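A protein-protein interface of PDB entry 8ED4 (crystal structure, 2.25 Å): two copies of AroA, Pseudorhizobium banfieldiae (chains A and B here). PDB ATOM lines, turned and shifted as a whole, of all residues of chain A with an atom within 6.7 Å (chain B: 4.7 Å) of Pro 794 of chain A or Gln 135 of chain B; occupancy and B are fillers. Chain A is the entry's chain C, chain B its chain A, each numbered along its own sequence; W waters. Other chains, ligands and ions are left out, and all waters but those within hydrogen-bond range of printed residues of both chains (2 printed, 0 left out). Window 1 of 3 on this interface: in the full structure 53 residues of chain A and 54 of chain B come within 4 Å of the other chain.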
ATOM      1  N   LYS A 490      14.775  25.781  -8.931  1.00  0.00           N
ATOM      2  CA  LYS A 490      15.119  25.016  -7.704  1.00  0.00           C
ATOM      3  C   LYS A 490      14.036  23.993  -7.319  1.00  0.00           C
ATOM      4  O   LYS A 490      14.372  23.047  -6.591  1.00  0.00           O
ATOM      5  CB  LYS A 490      15.289  25.975  -6.530  1.00  0.00           C
ATOM      6  CG  LYS A 490      16.515  26.865  -6.607  1.00  0.00           C
ATOM      7  CD  LYS A 490      16.713  27.713  -5.359  1.00  0.00           C
ATOM      8  CE  LYS A 490      15.695  28.828  -5.251  1.00  0.00           C
ATOM      9  NZ  LYS A 490      15.967  29.701  -4.086  1.00  0.00           N
ATOM     10  N   LYS A 548      16.698  32.321  -8.909  1.00  0.00           N
ATOM     11  CA  LYS A 548      17.510  31.545  -9.882  1.00  0.00           C
ATOM     12  C   LYS A 548      16.866  31.643 -11.266  1.00  0.00           C
ATOM     13  O   LYS A 548      17.591  31.894 -12.239  1.00  0.00           O
ATOM     14  CB  LYS A 548      17.652  30.104  -9.391  1.00  0.00           C
ATOM     15  CG  LYS A 548      18.411  29.974  -8.080  1.00  0.00           C
ATOM     16  CD  LYS A 548      19.798  30.606  -8.127  1.00  0.00           C
ATOM     17  CE  LYS A 548      20.660  30.212  -6.947  1.00  0.00           C
ATOM     18  NZ  LYS A 548      22.091  30.474  -7.229  1.00  0.00           N
ATOM     19  N   VAL A 723      16.127  24.447   7.308  1.00  0.00           N
ATOM     20  CA  VAL A 723      15.945  25.149   6.018  1.00  0.00           C
ATOM     21  C   VAL A 723      14.463  25.468   5.801  1.00  0.00           C
ATOM     22  O   VAL A 723      13.627  24.546   5.875  1.00  0.00           O
ATOM     23  CB  VAL A 723      16.508  24.291   4.881  1.00  0.00           C
ATOM     24  CG1 VAL A 723      16.296  24.995   3.546  1.00  0.00           C
ATOM     25  CG2 VAL A 723      17.972  23.951   5.126  1.00  0.00           C
ATOM     26  N   GLN A 725      12.054  26.096   2.928  1.00  0.00           N
ATOM     27  CA  GLN A 725      11.718  26.018   1.487  1.00  0.00           C
ATOM     28  C   GLN A 725      13.022  26.070   0.675  1.00  0.00           C
ATOM     29  O   GLN A 725      13.949  25.343   1.049  1.00  0.00           O
ATOM     30  CB  GLN A 725      10.683  27.114   1.223  1.00  0.00           C
ATOM     31  CG  GLN A 725       9.323  26.774   1.798  1.00  0.00           C
ATOM     32  CD  GLN A 725       8.706  25.655   0.994  1.00  0.00           C
ATOM     33  OE1 GLN A 725       8.847  24.483   1.326  1.00  0.00           O
ATOM     34  NE2 GLN A 725       8.072  26.012  -0.114  1.00  0.00           N
ATOM     35  N   SER A 726      13.116  26.905  -0.371  1.00  0.00           N
ATOM     36  CA  SER A 726      14.250  26.948  -1.339  1.00  0.00           C
ATOM     37  C   SER A 726      15.378  27.840  -0.806  1.00  0.00           C
ATOM     38  O   SER A 726      16.224  28.270  -1.611  1.00  0.00           O
ATOM     39  CB  SER A 726      13.797  27.399  -2.708  1.00  0.00           C
ATOM     40  OG  SER A 726      13.526  28.798  -2.737  1.00  0.00           O
ATOM     41  N   ALA A 727      15.393  28.117   0.499  1.00  0.00           N
ATOM     42  CA  ALA A 727      16.451  28.901   1.172  1.00  0.00           C
ATOM     43  C   ALA A 727      16.568  30.296   0.536  1.00  0.00           C
ATOM     44  O   ALA A 727      17.681  30.843   0.475  1.00  0.00           O
ATOM     45  CB  ALA A 727      17.753  28.139   1.095  1.00  0.00           C
ATOM     46  N   TYR A 728      15.449  30.873   0.096  1.00  0.00           N
ATOM     47  CA  TYR A 728      15.431  32.227  -0.512  1.00  0.00           C
ATOM     48  C   TYR A 728      15.920  33.252   0.529  1.00  0.00           C
ATOM     49  O   TYR A 728      16.742  34.117   0.178  1.00  0.00           O
ATOM     50  CB  TYR A 728      14.069  32.517  -1.153  1.00  0.00           C
ATOM     51  CG  TYR A 728      12.857  32.503  -0.256  1.00  0.00           C
ATOM     52  CD1 TYR A 728      12.434  33.650   0.390  1.00  0.00           C
ATOM     53  CD2 TYR A 728      12.089  31.365  -0.107  1.00  0.00           C
ATOM     54  CE1 TYR A 728      11.298  33.659   1.187  1.00  0.00           C
ATOM     55  CE2 TYR A 728      10.952  31.355   0.682  1.00  0.00           C
ATOM     56  CZ  TYR A 728      10.543  32.510   1.321  1.00  0.00           C
ATOM     57  OH  TYR A 728       9.427  32.513   2.100  1.00  0.00           O
ATOM     58  N   GLN A 731      19.683  31.584   2.444  1.00  0.00           N
ATOM     59  CA  GLN A 731      20.975  31.638   1.692  1.00  0.00           C
ATOM     60  C   GLN A 731      21.784  32.879   2.100  1.00  0.00           C
ATOM     61  O   GLN A 731      22.958  32.936   1.735  1.00  0.00           O
ATOM     62  CB  GLN A 731      20.750  31.556   0.174  1.00  0.00           C
ATOM     63  CG  GLN A 731      20.020  32.747  -0.436  1.00  0.00           C
ATOM     64  CD  GLN A 731      19.778  32.599  -1.922  1.00  0.00           C
ATOM     65  OE1 GLN A 731      20.173  31.623  -2.566  1.00  0.00           O
ATOM     66  NE2 GLN A 731      19.132  33.608  -2.478  1.00  0.00           N
ATOM     67  N   MET A 737      23.271  28.530   6.690  1.00  0.00           N
ATOM     68  CA  MET A 737      24.307  28.193   5.675  1.00  0.00           C
ATOM     69  C   MET A 737      25.564  27.652   6.383  1.00  0.00           C
ATOM     70  O   MET A 737      26.289  26.836   5.753  1.00  0.00           O
ATOM     71  CB  MET A 737      24.675  29.408   4.808  1.00  0.00           C
ATOM     72  CG  MET A 737      23.608  29.821   3.782  1.00  0.00           C
ATOM     73  SD  MET A 737      22.924  28.462   2.773  1.00  0.00           S
ATOM     74  CE  MET A 737      21.428  28.112   3.692  1.00  0.00           C
ATOM     75  N   TYR A 742      26.009  22.948   1.623  1.00  0.00           N
ATOM     76  CA  TYR A 742      25.519  22.048   0.553  1.00  0.00           C
ATOM     77  C   TYR A 742      24.260  21.354   1.055  1.00  0.00           C
ATOM     78  O   TYR A 742      24.117  21.126   2.255  1.00  0.00           O
ATOM     79  CB  TYR A 742      26.577  21.009   0.176  1.00  0.00           C
ATOM     80  CG  TYR A 742      27.788  21.536  -0.553  1.00  0.00           C
ATOM     81  CD1 TYR A 742      28.897  21.996   0.139  1.00  0.00           C
ATOM     82  CD2 TYR A 742      27.845  21.537  -1.933  1.00  0.00           C
ATOM     83  CE1 TYR A 742      30.020  22.460  -0.517  1.00  0.00           C
ATOM     84  CE2 TYR A 742      28.957  22.013  -2.608  1.00  0.00           C
ATOM     85  CZ  TYR A 742      30.054  22.472  -1.897  1.00  0.00           C
ATOM     86  OH  TYR A 742      31.168  22.920  -2.556  1.00  0.00           O
ATOM     87  N   PRO A 743      23.330  20.968   0.153  1.00  0.00           N
ATOM     88  CA  PRO A 743      22.194  20.140   0.550  1.00  0.00           C
ATOM     89  C   PRO A 743      22.781  18.779   0.943  1.00  0.00           C
ATOM     90  O   PRO A 743      23.623  18.248   0.210  1.00  0.00           O
ATOM     91  CB  PRO A 743      21.347  20.041  -0.720  1.00  0.00           C
ATOM     92  CG  PRO A 743      22.406  20.101  -1.814  1.00  0.00           C
ATOM     93  CD  PRO A 743      23.404  21.132  -1.310  1.00  0.00           C
ATOM     94  N   THR A 772      22.619  16.308 -10.608  1.00  0.00           N
ATOM     95  CA  THR A 772      22.748  17.360  -9.575  1.00  0.00           C
ATOM     96  C   THR A 772      23.809  16.914  -8.573  1.00  0.00           C
ATOM     97  O   THR A 772      24.414  15.851  -8.791  1.00  0.00           O
ATOM     98  CB  THR A 772      21.388  17.651  -8.935  1.00  0.00           C
ATOM     99  OG1 THR A 772      21.497  18.834  -8.137  1.00  0.00           O
ATOM    100  CG2 THR A 772      20.876  16.491  -8.108  1.00  0.00           C
ATOM    101  N   GLN A 773      24.016  17.703  -7.522  1.00  0.00           N
ATOM    102  CA  GLN A 773      25.106  17.489  -6.551  1.00  0.00           C
ATOM    103  C   GLN A 773      24.540  17.594  -5.135  1.00  0.00           C
ATOM    104  O   GLN A 773      23.548  18.291  -4.921  1.00  0.00           O
ATOM    105  CB  GLN A 773      26.255  18.463  -6.847  1.00  0.00           C
ATOM    106  CG  GLN A 773      25.939  19.931  -6.562  1.00  0.00           C
ATOM    107  CD  GLN A 773      27.148  20.831  -6.699  1.00  0.00           C
ATOM    108  OE1 GLN A 773      27.948  20.693  -7.622  1.00  0.00           O
ATOM    109  NE2 GLN A 773      27.281  21.779  -5.783  1.00  0.00           N
ATOM    110  N   PHE A 791      15.512  19.011  -0.610  1.00  0.00           N
ATOM    111  CA  PHE A 791      14.901  19.512  -1.869  1.00  0.00           C
ATOM    112  C   PHE A 791      15.143  21.024  -1.994  1.00  0.00           C
ATOM    113  O   PHE A 791      15.440  21.664  -0.950  1.00  0.00           O
ATOM    114  CB  PHE A 791      13.393  19.220  -1.905  1.00  0.00           C
ATOM    115  CG  PHE A 791      12.518  20.360  -1.441  1.00  0.00           C
ATOM    116  CD1 PHE A 791      12.466  20.720  -0.106  1.00  0.00           C
ATOM    117  CD2 PHE A 791      11.771  21.091  -2.348  1.00  0.00           C
ATOM    118  CE1 PHE A 791      11.672  21.778   0.316  1.00  0.00           C
ATOM    119  CE2 PHE A 791      10.971  22.138  -1.924  1.00  0.00           C
ATOM    120  CZ  PHE A 791      10.923  22.482  -0.593  1.00  0.00           C
ATOM    121  N   GLY A 792      14.970  21.560  -3.216  1.00  0.00           N
ATOM    122  CA  GLY A 792      14.787  22.997  -3.510  1.00  0.00           C
ATOM    123  C   GLY A 792      15.995  23.854  -3.153  1.00  0.00           C
ATOM    124  O   GLY A 792      15.840  25.089  -3.029  1.00  0.00           O
ATOM    125  N   PHE A 793      17.167  23.248  -2.979  1.00  0.00           N
ATOM    126  CA  PHE A 793      18.338  23.914  -2.353  1.00  0.00           C
ATOM    127  C   PHE A 793      19.231  24.543  -3.422  1.00  0.00           C
ATOM    128  O   PHE A 793      19.581  23.896  -4.407  1.00  0.00           O
ATOM    129  CB  PHE A 793      19.084  22.935  -1.457  1.00  0.00           C
ATOM    130  CG  PHE A 793      19.792  23.608  -0.312  1.00  0.00           C
ATOM    131  CD1 PHE A 793      19.072  24.129   0.751  1.00  0.00           C
ATOM    132  CD2 PHE A 793      21.171  23.739  -0.310  1.00  0.00           C
ATOM    133  CE1 PHE A 793      19.722  24.743   1.811  1.00  0.00           C
ATOM    134  CE2 PHE A 793      21.818  24.372   0.740  1.00  0.00           C
ATOM    135  CZ  PHE A 793      21.095  24.863   1.805  1.00  0.00           C
ATOM    136  N   PRO A 794      19.618  25.833  -3.258  1.00  0.00           N
ATOM    137  CA  PRO A 794      20.320  26.571  -4.315  1.00  0.00           C
ATOM    138  C   PRO A 794      21.663  25.941  -4.692  1.00  0.00           C
ATOM    139  O   PRO A 794      22.008  25.991  -5.836  1.00  0.00           O
ATOM    140  CB  PRO A 794      20.519  27.988  -3.749  1.00  0.00           C
ATOM    141  CG  PRO A 794      20.293  27.850  -2.257  1.00  0.00           C
ATOM    142  CD  PRO A 794      19.351  26.674  -2.083  1.00  0.00           C
ATOM    143  N   THR A 795      22.348  25.322  -3.729  1.00  0.00           N
ATOM    144  CA  THR A 795      23.729  24.796  -3.914  1.00  0.00           C
ATOM    145  C   THR A 795      23.703  23.316  -4.311  1.00  0.00           C
ATOM    146  O   THR A 795      24.779  22.693  -4.273  1.00  0.00           O
ATOM    147  CB  THR A 795      24.582  25.058  -2.672  1.00  0.00           C
ATOM    148  OG1 THR A 795      23.994  24.388  -1.558  1.00  0.00           O
ATOM    149  CG2 THR A 795      24.714  26.544  -2.403  1.00  0.00           C
ATOM    150  N   GLY A 796      22.529  22.805  -4.695  1.00  0.00           N
ATOM    151  CA  GLY A 796      22.331  21.464  -5.272  1.00  0.00           C
ATOM    152  C   GLY A 796      20.852  21.147  -5.351  1.00  0.00           C
ATOM    153  O   GLY A 796      20.259  20.918  -4.290  1.00  0.00           O
ATOM    154  N   VAL A 797      20.283  21.169  -6.560  1.00  0.00           N
ATOM    155  CA  VAL A 797      18.816  21.104  -6.819  1.00  0.00           C
ATOM    156  C   VAL A 797      18.426  19.648  -7.071  1.00  0.00           C
ATOM    157  O   VAL A 797      18.818  19.112  -8.143  1.00  0.00           O
ATOM    158  CB  VAL A 797      18.399  22.008  -7.999  1.00  0.00           C
ATOM    159  CG1 VAL A 797      16.894  21.975  -8.242  1.00  0.00           C
ATOM    160  CG2 VAL A 797      18.860  23.443  -7.798  1.00  0.00           C
ATOM    161  N   ASN A 800      16.466  18.189 -10.388  1.00  0.00           N
ATOM    162  CA  ASN A 800      17.185  17.922 -11.660  1.00  0.00           C
ATOM    163  C   ASN A 800      17.046  16.449 -12.035  1.00  0.00           C
ATOM    164  O   ASN A 800      17.081  16.158 -13.247  1.00  0.00           O
ATOM    165  CB  ASN A 800      18.660  18.321 -11.573  1.00  0.00           C
ATOM    166  CG  ASN A 800      18.897  19.817 -11.663  1.00  0.00           C
ATOM    167  OD1 ASN A 800      18.083  20.621 -11.202  1.00  0.00           O
ATOM    168  ND2 ASN A 800      20.017  20.200 -12.247  1.00  0.00           N
ATOM    169  N   PRO B 126      34.938  28.333  -4.691  1.00  0.00           N
ATOM    170  CA  PRO B 126      34.936  28.116  -6.136  1.00  0.00           C
ATOM    171  C   PRO B 126      33.514  27.793  -6.612  1.00  0.00           C
ATOM    172  O   PRO B 126      32.808  27.133  -5.876  1.00  0.00           O
ATOM    173  CB  PRO B 126      35.855  26.904  -6.359  1.00  0.00           C
ATOM    174  CG  PRO B 126      36.753  26.902  -5.156  1.00  0.00           C
ATOM    175  CD  PRO B 126      35.929  27.488  -4.021  1.00  0.00           C
ATOM    176  N   LEU B 127      33.148  28.285  -7.799  1.00  0.00           N
ATOM    177  CA  LEU B 127      31.843  28.050  -8.467  1.00  0.00           C
ATOM    178  C   LEU B 127      32.111  27.502  -9.868  1.00  0.00           C
ATOM    179  O   LEU B 127      33.063  27.963 -10.507  1.00  0.00           O
ATOM    180  CB  LEU B 127      31.075  29.364  -8.565  1.00  0.00           C
ATOM    181  CG  LEU B 127      30.835  30.107  -7.260  1.00  0.00           C
ATOM    182  CD1 LEU B 127      30.182  31.454  -7.521  1.00  0.00           C
ATOM    183  CD2 LEU B 127      29.985  29.282  -6.315  1.00  0.00           C
ATOM    184  N   VAL B 128      31.289  26.554 -10.314  1.00  0.00           N
ATOM    185  CA  VAL B 128      31.310  26.030 -11.707  1.00  0.00           C
ATOM    186  C   VAL B 128      29.877  26.001 -12.228  1.00  0.00           C
ATOM    187  O   VAL B 128      28.958  25.633 -11.471  1.00  0.00           O
ATOM    188  CB  VAL B 128      31.954  24.636 -11.798  1.00  0.00           C
ATOM    189  CG1 VAL B 128      31.915  24.086 -13.218  1.00  0.00           C
ATOM    190  CG2 VAL B 128      33.372  24.632 -11.259  1.00  0.00           C
ATOM    191  N   ARG B 130      27.276  24.140 -13.861  1.00  0.00           N
ATOM    192  CA  ARG B 130      26.800  22.748 -14.083  1.00  0.00           C
ATOM    193  C   ARG B 130      25.373  22.576 -13.540  1.00  0.00           C
ATOM    194  O   ARG B 130      25.009  23.222 -12.545  1.00  0.00           O
ATOM    195  CB  ARG B 130      27.772  21.750 -13.452  1.00  0.00           C
ATOM    196  CG  ARG B 130      28.057  21.983 -11.977  1.00  0.00           C
ATOM    197  CD  ARG B 130      29.086  20.936 -11.572  1.00  0.00           C
ATOM    198  NE  ARG B 130      29.317  20.820 -10.129  1.00  0.00           N
ATOM    199  CZ  ARG B 130      30.500  20.850  -9.535  1.00  0.00           C
ATOM    200  NH1 ARG B 130      31.603  21.017 -10.239  1.00  0.00           N
ATOM    201  NH2 ARG B 130      30.579  20.710  -8.227  1.00  0.00           N
ATOM    202  N   TYR B 131      24.585  21.726 -14.191  1.00  0.00           N
ATOM    203  CA  TYR B 131      23.210  21.378 -13.751  1.00  0.00           C
ATOM    204  C   TYR B 131      22.300  22.610 -13.869  1.00  0.00           C
ATOM    205  O   TYR B 131      21.307  22.684 -13.135  1.00  0.00           O
ATOM    206  CB  TYR B 131      23.240  20.831 -12.319  1.00  0.00           C
ATOM    207  CG  TYR B 131      24.349  19.846 -12.028  1.00  0.00           C
ATOM    208  CD1 TYR B 131      24.592  18.766 -12.866  1.00  0.00           C
ATOM    209  CD2 TYR B 131      25.142  19.970 -10.899  1.00  0.00           C
ATOM    210  CE1 TYR B 131      25.596  17.849 -12.594  1.00  0.00           C
ATOM    211  CE2 TYR B 131      26.147  19.053 -10.613  1.00  0.00           C
ATOM    212  CZ  TYR B 131      26.380  17.994 -11.468  1.00  0.00           C
ATOM    213  OH  TYR B 131      27.381  17.105 -11.210  1.00  0.00           O
ATOM    214  N   GLN B 133      22.940  26.009 -13.559  1.00  0.00           N
ATOM    215  CA  GLN B 133      23.315  27.258 -12.847  1.00  0.00           C
ATOM    216  C   GLN B 133      24.716  27.117 -12.251  1.00  0.00           C
ATOM    217  O   GLN B 133      25.309  26.037 -12.386  1.00  0.00           O
ATOM    218  CB  GLN B 133      22.298  27.625 -11.765  1.00  0.00           C
ATOM    219  CG  GLN B 133      22.309  26.723 -10.541  1.00  0.00           C
ATOM    220  CD  GLN B 133      21.098  25.824 -10.512  1.00  0.00           C
ATOM    221  OE1 GLN B 133      21.137  24.682 -10.997  1.00  0.00           O
ATOM    222  NE2 GLN B 133      20.007  26.341  -9.954  1.00  0.00           N
ATOM    223  N   MET B 134      25.231  28.187 -11.646  1.00  0.00           N
ATOM    224  CA  MET B 134      26.543  28.161 -10.955  1.00  0.00           C
ATOM    225  C   MET B 134      26.377  27.335  -9.681  1.00  0.00           C
ATOM    226  O   MET B 134      25.340  27.484  -9.027  1.00  0.00           O
ATOM    227  CB  MET B 134      27.041  29.566 -10.594  1.00  0.00           C
ATOM    228  CG  MET B 134      27.530  30.366 -11.789  1.00  0.00           C
ATOM    229  SD  MET B 134      28.716  29.471 -12.835  1.00  0.00           S
ATOM    230  CE  MET B 134      30.275  30.040 -12.161  1.00  0.00           C
ATOM    231  N   GLN B 135      27.355  26.485  -9.384  1.00  0.00           N
ATOM    232  CA  GLN B 135      27.298  25.584  -8.210  1.00  0.00           C
ATOM    233  C   GLN B 135      28.626  25.676  -7.471  1.00  0.00           C
ATOM    234  O   GLN B 135      29.686  25.691  -8.086  1.00  0.00           O
ATOM    235  CB  GLN B 135      26.975  24.159  -8.659  1.00  0.00           C
ATOM    236  CG  GLN B 135      25.604  23.998  -9.305  1.00  0.00           C
ATOM    237  CD  GLN B 135      24.471  23.855  -8.314  1.00  0.00           C
ATOM    238  OE1 GLN B 135      23.976  22.755  -8.088  1.00  0.00           O
ATOM    239  NE2 GLN B 135      24.032  24.966  -7.734  1.00  0.00           N
ATOM    240  N   PRO B 136      28.617  25.755  -6.128  1.00  0.00           N
ATOM    241  CA  PRO B 136      29.861  25.744  -5.372  1.00  0.00           C
ATOM    242  C   PRO B 136      30.504  24.350  -5.472  1.00  0.00           C
ATOM    243  O   PRO B 136      29.800  23.357  -5.650  1.00  0.00           O
ATOM    244  CB  PRO B 136      29.451  26.159  -3.953  1.00  0.00           C
ATOM    245  CG  PRO B 136      27.976  25.852  -3.858  1.00  0.00           C
ATOM    246  CD  PRO B 136      27.430  25.836  -5.273  1.00  0.00           C
ATOM    247  N   THR B 137      31.835  24.317  -5.452  1.00  0.00           N
ATOM    248  CA  THR B 137      32.647  23.078  -5.518  1.00  0.00           C
ATOM    249  C   THR B 137      33.982  23.313  -4.803  1.00  0.00           C
ATOM    250  O   THR B 137      34.189  24.411  -4.241  1.00  0.00           O
ATOM    251  CB  THR B 137      32.823  22.619  -6.971  1.00  0.00           C
ATOM    252  OG1 THR B 137      33.359  21.296  -6.970  1.00  0.00           O
ATOM    253  CG2 THR B 137      33.731  23.515  -7.779  1.00  0.00           C
HETATM  254  O   HOH W   1      21.830  21.499  -8.859  1.00  0.00           O
HETATM  255  O   HOH W   2      33.046  24.725  -1.384  1.00  0.00           O
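The backbone carbonyl oxygen of Tyr 131 of chain B sits at hydrogen-bond distance from the side-chain amide nitrogen of Asn 800 of chain A. O of Pro 136 of chain B lies close to OH of Tyr 742 of chain A. The guanidinium group of Arg 130 of chain B sits at hydrogen-bond distance from the side-chain amide oxygen of Gln 773 of chain A, 2.7 Å away. N of Thr 137 of chain B is in hydrogen-bond range of OH of Tyr 742 of chain A (3.3 Å). O of Pro 136 of chain B sits at hydrogen-bond distance from NE2 of Gln 773 of chain A (3.0 Å). NE2 of Gln 135 of chain B sits at hydrogen-bond distance from O of Pro 794 of chain A, 3.0 Å away.
Val 723 of chain A touches none of the printed residues of chain B. Printed residues of chain B within 4 Å of Thr 772 of chain A: Tyr 131. Of chain B, only Gln 135 (3.0 Å) comes within 4 Å of Pro 794 of chain A. Printed residues of chain B within 4 Å of Asn 800 of chain A: Tyr 131. Val 128 of chain B touches none of the printed residues of chain A. Printed residues of chain A within 4 Å of Gln 133 of chain B: Val 797 (3.8 Å). Gln 135 of chain B touches four residues of chain A. Of the printed residues of chain A, Thr 137 of chain B touches Tyr 742 (3.3 Å). The nearest printed residue of chain B that does not touch Gly 796 of chain A is Pro 136 of chain B (5.8 Å).
No position is printed for both chains.
Among the printed residues, merely in contact across the chains: Gly 796 of chain A with Gln 135 of chain B, Thr 795 of chain A with Pro 136 of chain B, Gln 773 of chain A with Gln 135 of chain B, Thr 772 of chain A with Tyr 131 of chain B, Val 797 of chain A with Gln 133 of chain B, Gln 773 of chain A with Tyr 131 of chain B and Thr 795 of chain A with Gln 135 of chain B.
Of the 10 printed residues of chain B, 6 touch a printed residue of chain A. Hydrophobic or aromatic side chains of chain B within 4 Å of the printed part of chain A: Tyr 131 and Pro 136. Among the printed residues, no Asp or Glu carboxylate lies within 4 Å of a Lys or Arg side-chain nitrogen of the other chain.
The backbone carbonyl oxygen (O) of Val 797 of chain A is in hydrogen-bond range of the side-chain hydroxyl (OG1) of Thr 772 of chain A, at 2.7 Å. OE1 of Gln 133 of chain B lies close to O of Tyr 131 of chain B (2.9 Å). OG1 of Thr 137 of chain B lies within hydrogen-bond range of NH2 of Arg 130 of chain B (3.1 Å). The side-chain amide oxygen (OD1) of Asn 800 of chain A lies close to the backbone carbonyl oxygen (O) of Val 797 of chain A, at 3.5 Å. The backbone carbonyl oxygen of Val 128 of chain B lies within hydrogen-bond range of the backbone NH of Gln 135 of chain B (2.8 Å). The side-chain amide nitrogen of Gln 773 of chain A lies within hydrogen-bond range of the backbone carbonyl oxygen of Thr 795 of chain A (3.1 Å).
Water W1 lies within hydrogen-bond range of the side-chain amide oxygen of Gln 135 of chain B, the side-chain hydroxyl of Thr 772 of chain A and the backbone NH of Val 797 of chain A. Water W2 lies within hydrogen-bond range of OH of Tyr 742 of chain A (2.9 Å) and O of Thr 137 of chain B (3.1 Å).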
